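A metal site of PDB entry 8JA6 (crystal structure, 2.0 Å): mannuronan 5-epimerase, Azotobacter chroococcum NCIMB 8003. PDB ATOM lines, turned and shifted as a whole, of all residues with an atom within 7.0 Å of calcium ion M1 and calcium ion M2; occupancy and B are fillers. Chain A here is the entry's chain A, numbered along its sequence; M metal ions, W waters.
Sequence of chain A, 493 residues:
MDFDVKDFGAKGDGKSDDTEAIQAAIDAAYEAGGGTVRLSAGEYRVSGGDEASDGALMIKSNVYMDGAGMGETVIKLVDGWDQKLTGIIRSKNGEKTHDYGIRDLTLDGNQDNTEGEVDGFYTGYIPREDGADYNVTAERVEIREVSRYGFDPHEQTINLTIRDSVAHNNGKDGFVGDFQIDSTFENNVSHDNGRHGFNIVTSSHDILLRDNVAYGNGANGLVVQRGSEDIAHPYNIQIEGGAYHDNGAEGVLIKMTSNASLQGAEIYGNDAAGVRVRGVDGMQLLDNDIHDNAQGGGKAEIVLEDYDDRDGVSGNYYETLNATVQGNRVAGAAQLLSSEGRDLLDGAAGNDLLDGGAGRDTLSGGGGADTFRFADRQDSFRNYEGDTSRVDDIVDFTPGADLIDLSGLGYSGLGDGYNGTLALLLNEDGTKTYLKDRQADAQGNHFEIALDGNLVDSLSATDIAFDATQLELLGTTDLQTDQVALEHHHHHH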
ATOM      1  N   ASN A 322     -28.421  -6.843 -12.360  1.00  0.00           N
ATOM      2  CA  ASN A 322     -27.674  -7.258 -11.166  1.00  0.00           C
ATOM      3  C   ASN A 322     -26.233  -7.652 -11.507  1.00  0.00           C
ATOM      4  O   ASN A 322     -25.762  -8.747 -11.183  1.00  0.00           O
ATOM      5  CB  ASN A 322     -28.404  -8.387 -10.461  1.00  0.00           C
ATOM      6  CG  ASN A 322     -29.778  -7.951 -10.015  1.00  0.00           C
ATOM      7  OD1 ASN A 322     -29.918  -6.960  -9.294  1.00  0.00           O
ATOM      8  ND2 ASN A 322     -30.819  -8.673 -10.456  1.00  0.00           N
ATOM      9  N   SER A 338     -26.337  -2.144 -17.981  1.00  0.00           N
ATOM     10  CA  SER A 338     -27.277  -2.939 -17.200  1.00  0.00           C
ATOM     11  C   SER A 338     -28.575  -2.157 -17.026  1.00  0.00           C
ATOM     12  O   SER A 338     -28.769  -1.077 -17.599  1.00  0.00           O
ATOM     13  CB  SER A 338     -26.646  -3.335 -15.861  1.00  0.00           C
ATOM     14  OG  SER A 338     -27.391  -4.365 -15.235  1.00  0.00           O
ATOM     15  N   SER A 339     -29.459  -2.658 -16.175  1.00  0.00           N
ATOM     16  CA  SER A 339     -30.819  -2.129 -16.097  1.00  0.00           C
ATOM     17  C   SER A 339     -31.321  -2.177 -14.656  1.00  0.00           C
ATOM     18  O   SER A 339     -30.522  -1.978 -13.732  1.00  0.00           O
ATOM     19  CB  SER A 339     -31.754  -2.879 -17.041  1.00  0.00           C
ATOM     20  OG  SER A 339     -33.023  -2.265 -17.002  1.00  0.00           O
ATOM     21  N   GLU A 340     -32.644  -2.294 -14.458  1.00  0.00           N
ATOM     22  CA  GLU A 340     -33.249  -2.092 -13.133  1.00  0.00           C
ATOM     23  C   GLU A 340     -32.502  -2.845 -12.039  1.00  0.00           C
ATOM     24  O   GLU A 340     -32.158  -4.027 -12.195  1.00  0.00           O
ATOM     25  CB  GLU A 340     -34.723  -2.529 -13.131  1.00  0.00           C
ATOM     26  CG  GLU A 340     -35.321  -2.372 -11.706  1.00  0.00           C
ATOM     27  CD  GLU A 340     -35.429  -0.880 -11.292  1.00  0.00           C
ATOM     28  OE1 GLU A 340     -34.635  -0.391 -10.424  1.00  0.00           O
ATOM     29  OE2 GLU A 340     -36.339  -0.210 -11.836  1.00  0.00           O
ATOM     30  N   GLY A 341     -32.243  -2.154 -10.933  1.00  0.00           N
ATOM     31  CA  GLY A 341     -31.525  -2.704  -9.792  1.00  0.00           C
ATOM     32  C   GLY A 341     -30.131  -2.115  -9.679  1.00  0.00           C
ATOM     33  O   GLY A 341     -29.691  -1.330 -10.516  1.00  0.00           O
ATOM     34  N   ARG A 342     -29.440  -2.518  -8.625  1.00  0.00           N
ATOM     35  CA  ARG A 342     -28.150  -1.916  -8.285  1.00  0.00           C
ATOM     36  C   ARG A 342     -27.045  -2.628  -9.043  1.00  0.00           C
ATOM     37  O   ARG A 342     -26.849  -3.833  -8.877  1.00  0.00           O
ATOM     38  CB  ARG A 342     -27.900  -1.981  -6.775  1.00  0.00           C
ATOM     39  CG  ARG A 342     -26.479  -1.533  -6.372  1.00  0.00           C
ATOM     40  CD  ARG A 342     -26.555  -0.651  -5.126  1.00  0.00           C
ATOM     41  NE  ARG A 342     -25.227  -0.325  -4.614  1.00  0.00           N
ATOM     42  CZ  ARG A 342     -24.453   0.634  -5.118  1.00  0.00           C
ATOM     43  NH1 ARG A 342     -24.831   1.349  -6.172  1.00  0.00           N
ATOM     44  NH2 ARG A 342     -23.268   0.877  -4.562  1.00  0.00           N
ATOM     45  N   ASP A 343     -26.301  -1.878  -9.852  1.00  0.00           N
ATOM     46  CA  ASP A 343     -25.134  -2.381 -10.566  1.00  0.00           C
ATOM     47  C   ASP A 343     -23.866  -1.694 -10.097  1.00  0.00           C
ATOM     48  O   ASP A 343     -23.867  -0.488  -9.837  1.00  0.00           O
ATOM     49  CB  ASP A 343     -25.320  -2.175 -12.071  1.00  0.00           C
ATOM     50  CG  ASP A 343     -26.543  -2.904 -12.579  1.00  0.00           C
ATOM     51  OD1 ASP A 343     -26.442  -4.133 -12.807  1.00  0.00           O
ATOM     52  OD2 ASP A 343     -27.603  -2.271 -12.685  1.00  0.00           O
ATOM     53  N   LEU A 345     -20.261  -1.179 -11.648  1.00  0.00           N
ATOM     54  CA  LEU A 345     -19.626  -1.313 -12.960  1.00  0.00           C
ATOM     55  C   LEU A 345     -18.312  -0.548 -12.953  1.00  0.00           C
ATOM     56  O   LEU A 345     -18.308   0.691 -12.905  1.00  0.00           O
ATOM     57  CB  LEU A 345     -20.563  -0.816 -14.062  1.00  0.00           C
ATOM     58  CG  LEU A 345     -21.957  -1.464 -14.101  1.00  0.00           C
ATOM     59  CD1 LEU A 345     -22.881  -0.776 -15.088  1.00  0.00           C
ATOM     60  CD2 LEU A 345     -21.894  -2.967 -14.414  1.00  0.00           C
ATOM     61  N   ASP A 355     -23.201   2.322 -18.305  1.00  0.00           N
ATOM     62  CA  ASP A 355     -24.582   2.767 -18.106  1.00  0.00           C
ATOM     63  C   ASP A 355     -25.261   1.737 -17.231  1.00  0.00           C
ATOM     64  O   ASP A 355     -25.583   0.639 -17.706  1.00  0.00           O
ATOM     65  CB  ASP A 355     -25.320   2.944 -19.429  1.00  0.00           C
ATOM     66  CG  ASP A 355     -26.732   3.544 -19.245  1.00  0.00           C
ATOM     67  OD1 ASP A 355     -27.217   3.638 -18.100  1.00  0.00           O
ATOM     68  OD2 ASP A 355     -27.338   3.940 -20.269  1.00  0.00           O
ATOM     69  N   GLY A 356     -25.519   2.084 -15.980  1.00  0.00           N
ATOM     70  CA  GLY A 356     -26.219   1.133 -15.139  1.00  0.00           C
ATOM     71  C   GLY A 356     -27.731   1.122 -15.286  1.00  0.00           C
ATOM     72  O   GLY A 356     -28.378   0.308 -14.612  1.00  0.00           O
ATOM     73  N   GLY A 357     -28.314   1.993 -16.117  1.00  0.00           N
ATOM     74  CA  GLY A 357     -29.764   1.954 -16.318  1.00  0.00           C
ATOM     75  C   GLY A 357     -30.532   2.335 -15.048  1.00  0.00           C
ATOM     76  O   GLY A 357     -30.049   3.088 -14.199  1.00  0.00           O
ATOM     77  N   ALA A 358     -31.751   1.820 -14.920  1.00  0.00           N
ATOM     78  CA  ALA A 358     -32.556   2.127 -13.743  1.00  0.00           C
ATOM     79  C   ALA A 358     -31.875   1.629 -12.463  1.00  0.00           C
ATOM     80  O   ALA A 358     -30.953   0.798 -12.497  1.00  0.00           O
ATOM     81  CB  ALA A 358     -33.966   1.530 -13.873  1.00  0.00           C
ATOM     82  N   GLY A 359     -32.295   2.193 -11.336  1.00  0.00           N
ATOM     83  CA  GLY A 359     -31.748   1.810 -10.050  1.00  0.00           C
ATOM     84  C   GLY A 359     -30.468   2.565  -9.739  1.00  0.00           C
ATOM     85  O   GLY A 359     -29.908   3.299 -10.571  1.00  0.00           O
ATOM     86  N   ARG A 360     -29.969   2.353  -8.521  1.00  0.00           N
ATOM     87  CA  ARG A 360     -28.824   3.105  -8.007  1.00  0.00           C
ATOM     88  C   ARG A 360     -27.543   2.348  -8.328  1.00  0.00           C
ATOM     89  O   ARG A 360     -27.277   1.282  -7.756  1.00  0.00           O
ATOM     90  CB  ARG A 360     -28.952   3.325  -6.502  1.00  0.00           C
ATOM     91  CG  ARG A 360     -27.745   4.086  -5.936  1.00  0.00           C
ATOM     92  CD  ARG A 360     -27.889   4.348  -4.468  1.00  0.00           C
ATOM     93  NE  ARG A 360     -27.513   3.188  -3.677  1.00  0.00           N
ATOM     94  CZ  ARG A 360     -26.285   2.947  -3.238  1.00  0.00           C
ATOM     95  NH1 ARG A 360     -25.272   3.735  -3.566  1.00  0.00           N
ATOM     96  NH2 ARG A 360     -26.064   1.882  -2.466  1.00  0.00           N
ATOM     97  N   ASP A 361     -26.747   2.905  -9.239  1.00  0.00           N
ATOM     98  CA  ASP A 361     -25.542   2.266  -9.716  1.00  0.00           C
ATOM     99  C   ASP A 361     -24.313   3.037  -9.248  1.00  0.00           C
ATOM    100  O   ASP A 361     -24.357   4.253  -9.066  1.00  0.00           O
ATOM    101  CB  ASP A 361     -25.561   2.183 -11.239  1.00  0.00           C
ATOM    102  CG  ASP A 361     -26.894   1.673 -11.734  1.00  0.00           C
ATOM    103  OD1 ASP A 361     -27.264   0.550 -11.324  1.00  0.00           O
ATOM    104  OD2 ASP A 361     -27.591   2.378 -12.487  1.00  0.00           O
ATOM    105  N   THR A 362     -23.213   2.314  -9.079  1.00  0.00           N
ATOM    106  CA  THR A 362     -21.916   2.913  -8.781  1.00  0.00           C
ATOM    107  C   THR A 362     -20.989   2.605  -9.932  1.00  0.00           C
ATOM    108  O   THR A 362     -20.762   1.422 -10.247  1.00  0.00           O
ATOM    109  CB  THR A 362     -21.353   2.389  -7.449  1.00  0.00           C
ATOM    110  OG1 THR A 362     -22.257   2.732  -6.389  1.00  0.00           O
ATOM    111  CG2 THR A 362     -20.005   3.029  -7.166  1.00  0.00           C
ATOM    112  N   LEU A 363     -20.469   3.648 -10.583  1.00  0.00           N
ATOM    113  CA  LEU A 363     -19.705   3.501 -11.816  1.00  0.00           C
ATOM    114  C   LEU A 363     -18.281   4.027 -11.634  1.00  0.00           C
ATOM    115  O   LEU A 363     -18.069   5.053 -10.967  1.00  0.00           O
ATOM    116  CB  LEU A 363     -20.370   4.247 -12.971  1.00  0.00           C
ATOM    117  CG  LEU A 363     -21.907   4.122 -13.042  1.00  0.00           C
ATOM    118  CD1 LEU A 363     -22.534   5.193 -13.906  1.00  0.00           C
ATOM    119  CD2 LEU A 363     -22.241   2.757 -13.576  1.00  0.00           C
ATOM    120  N   PHE A 374     -26.268   8.296 -19.240  1.00  0.00           N
ATOM    121  CA  PHE A 374     -27.517   8.339 -18.498  1.00  0.00           C
ATOM    122  C   PHE A 374     -28.627   8.461 -19.525  1.00  0.00           C
ATOM    123  O   PHE A 374     -28.815   9.533 -20.118  1.00  0.00           O
ATOM    124  CB  PHE A 374     -27.493   9.470 -17.467  1.00  0.00           C
ATOM    125  CG  PHE A 374     -26.459   9.273 -16.425  1.00  0.00           C
ATOM    126  CD1 PHE A 374     -26.778   8.698 -15.214  1.00  0.00           C
ATOM    127  CD2 PHE A 374     -25.132   9.600 -16.674  1.00  0.00           C
ATOM    128  CE1 PHE A 374     -25.800   8.459 -14.259  1.00  0.00           C
ATOM    129  CE2 PHE A 374     -24.154   9.364 -15.751  1.00  0.00           C
ATOM    130  CZ  PHE A 374     -24.490   8.798 -14.529  1.00  0.00           C
ATOM    131  N   GLN A 378     -35.139   9.076 -15.218  1.00  0.00           N
ATOM    132  CA  GLN A 378     -35.538   8.232 -14.099  1.00  0.00           C
ATOM    133  C   GLN A 378     -34.479   7.199 -13.720  1.00  0.00           C
ATOM    134  O   GLN A 378     -34.739   6.370 -12.838  1.00  0.00           O
ATOM    135  CB  GLN A 378     -36.864   7.524 -14.433  1.00  0.00           C
ATOM    136  CG  GLN A 378     -38.100   8.362 -14.155  1.00  0.00           C
ATOM    137  CD  GLN A 378     -38.280   8.688 -12.674  1.00  0.00           C
ATOM    138  OE1 GLN A 378     -38.004   9.809 -12.229  1.00  0.00           O
ATOM    139  NE2 GLN A 378     -38.778   7.707 -11.915  1.00  0.00           N
ATOM    140  N   ASP A 379     -33.308   7.191 -14.367  1.00  0.00           N
ATOM    141  CA  ASP A 379     -32.273   6.228 -14.019  1.00  0.00           C
ATOM    142  C   ASP A 379     -31.345   6.722 -12.902  1.00  0.00           C
ATOM    143  O   ASP A 379     -30.567   5.927 -12.369  1.00  0.00           O
ATOM    144  CB  ASP A 379     -31.448   5.873 -15.262  1.00  0.00           C
ATOM    145  CG  ASP A 379     -32.264   5.081 -16.305  1.00  0.00           C
ATOM    146  OD1 ASP A 379     -33.404   4.652 -16.010  1.00  0.00           O
ATOM    147  OD2 ASP A 379     -31.735   4.885 -17.426  1.00  0.00           O
ATOM    148  N   SER A 380     -31.431   7.994 -12.521  1.00  0.00           N
ATOM    149  CA  SER A 380     -30.609   8.549 -11.433  1.00  0.00           C
ATOM    150  C   SER A 380     -31.345   9.776 -10.926  1.00  0.00           C
ATOM    151  O   SER A 380     -31.402  10.785 -11.637  1.00  0.00           O
ATOM    152  CB  SER A 380     -29.211   8.892 -11.941  1.00  0.00           C
ATOM    153  OG  SER A 380     -28.319   9.262 -10.887  1.00  0.00           O
ATOM    154  N   PHE A 381     -31.943   9.685  -9.730  1.00  0.00           N
ATOM    155  CA  PHE A 381     -32.801  10.763  -9.271  1.00  0.00           C
ATOM    156  C   PHE A 381     -32.950  10.761  -7.751  1.00  0.00           C
ATOM    157  O   PHE A 381     -32.772   9.734  -7.083  1.00  0.00           O
ATOM    158  CB  PHE A 381     -34.186  10.696  -9.917  1.00  0.00           C
ATOM    159  CG  PHE A 381     -35.023   9.522  -9.445  1.00  0.00           C
ATOM    160  CD1 PHE A 381     -35.927   9.671  -8.399  1.00  0.00           C
ATOM    161  CD2 PHE A 381     -34.892   8.276 -10.043  1.00  0.00           C
ATOM    162  CE1 PHE A 381     -36.696   8.605  -7.958  1.00  0.00           C
ATOM    163  CE2 PHE A 381     -35.659   7.193  -9.619  1.00  0.00           C
ATOM    164  CZ  PHE A 381     -36.557   7.353  -8.566  1.00  0.00           C
ATOM    165  N   ARG A 390     -31.853   6.469  -4.929  1.00  0.00           N
ATOM    166  CA  ARG A 390     -31.829   6.155  -6.361  1.00  0.00           C
ATOM    167  C   ARG A 390     -30.888   7.075  -7.136  1.00  0.00           C
ATOM    168  O   ARG A 390     -31.001   7.172  -8.372  1.00  0.00           O
ATOM    169  CB  ARG A 390     -33.247   6.205  -6.953  1.00  0.00           C
ATOM    170  CG  ARG A 390     -34.263   5.341  -6.221  1.00  0.00           C
ATOM    171  CD  ARG A 390     -34.182   3.854  -6.529  1.00  0.00           C
ATOM    172  NE  ARG A 390     -34.428   3.520  -7.931  1.00  0.00           N
ATOM    173  CZ  ARG A 390     -35.580   3.097  -8.437  1.00  0.00           C
ATOM    174  NH1 ARG A 390     -36.687   3.066  -7.699  1.00  0.00           N
ATOM    175  NH2 ARG A 390     -35.621   2.695  -9.709  1.00  0.00           N
ATOM    176  N   VAL A 391     -29.939   7.738  -6.465  1.00  0.00           N
ATOM    177  CA  VAL A 391     -28.957   8.590  -7.130  1.00  0.00           C
ATOM    178  C   VAL A 391     -27.702   7.773  -7.425  1.00  0.00           C
ATOM    179  O   VAL A 391     -27.064   7.261  -6.496  1.00  0.00           O
ATOM    180  CB  VAL A 391     -28.621   9.828  -6.294  1.00  0.00           C
ATOM    181  CG1 VAL A 391     -27.527  10.638  -6.975  1.00  0.00           C
ATOM    182  CG2 VAL A 391     -29.865  10.675  -6.037  1.00  0.00           C
ATOM    183  N   ASP A 392     -27.331   7.682  -8.710  1.00  0.00           N
ATOM    184  CA  ASP A 392     -26.071   7.059  -9.115  1.00  0.00           C
ATOM    185  C   ASP A 392     -24.869   7.872  -8.661  1.00  0.00           C
ATOM    186  O   ASP A 392     -24.919   9.109  -8.586  1.00  0.00           O
ATOM    187  CB  ASP A 392     -25.968   6.933 -10.645  1.00  0.00           C
ATOM    188  CG  ASP A 392     -26.877   5.884 -11.226  1.00  0.00           C
ATOM    189  OD1 ASP A 392     -27.693   5.276 -10.507  1.00  0.00           O
ATOM    190  OD2 ASP A 392     -26.751   5.678 -12.456  1.00  0.00           O
HETATM  191 CA    CA M   1     -29.059  -0.457 -12.545  1.00  0.00          CA
HETATM  192 CA    CA M   2     -28.876   4.303 -12.546  1.00  0.00          CA
HETATM  193  O   HOH W   1     -28.167   5.416 -14.734  1.00  0.00           O
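Calcium ion M2 is bound by the side-chain carboxylate (OD2) of Asp 361 (2.3 Å), the backbone carbonyl oxygen (O) of Asp 379 (2.4 Å), the backbone carbonyl oxygen (O) of Gly 357 (2.4 Å), the backbone carbonyl oxygen (O) of Gly 359 (2.4 Å), the side-chain carboxylate (OD2) of Asp 392 (2.5 Å), the side-chain carboxylate (OD1) of Asp 392 (2.6 Å) and water W1 (2.6 Å).
OD1 of Asp 379 sits at hydrogen-bond distance from N of Ala 358 (3.5 Å). OG of Ser 380 sits at hydrogen-bond distance from N of Asp 392 (2.9 Å). The backbone NH of Gly 357 sits close to the backbone carbonyl oxygen of Ser 338 (3.4 Å). The side-chain carboxylate (OD1) of Asp 343 lies within hydrogen-bond range of the backbone NH (N) of Asn 322, 3.4 Å away. The side-chain carboxylate of Asp 355 sits at hydrogen-bond distance from the backbone NH of Gly 357. O of Asp 343 sits at hydrogen-bond distance from N of Thr 362, at 3.0 Å. The side-chain carboxylate of Asp 343 lies within hydrogen-bond range of the side-chain hydroxyl of Ser 338 (2.6 Å).
Five residues have an atom within 4 Å of calcium ion M2: Gly 357, Gly 359, Asp 361, Asp 379 and Asp 392.
The nearest printed residue that does not touch calcium ion M1 is Gly 357 (4.03 Å).
Calcium ion M1 is bound by O of Ala 358 (2.3 Å), O of Gly 341 (2.3 Å), O of Gly 356 (2.3 Å), OD2 of Asp 343 (2.3 Å), OD1 of Asp 361 (2.4 Å) and O of Ser 339 (2.4 Å). Calcium ion M1 has six donor atoms within binding distance.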
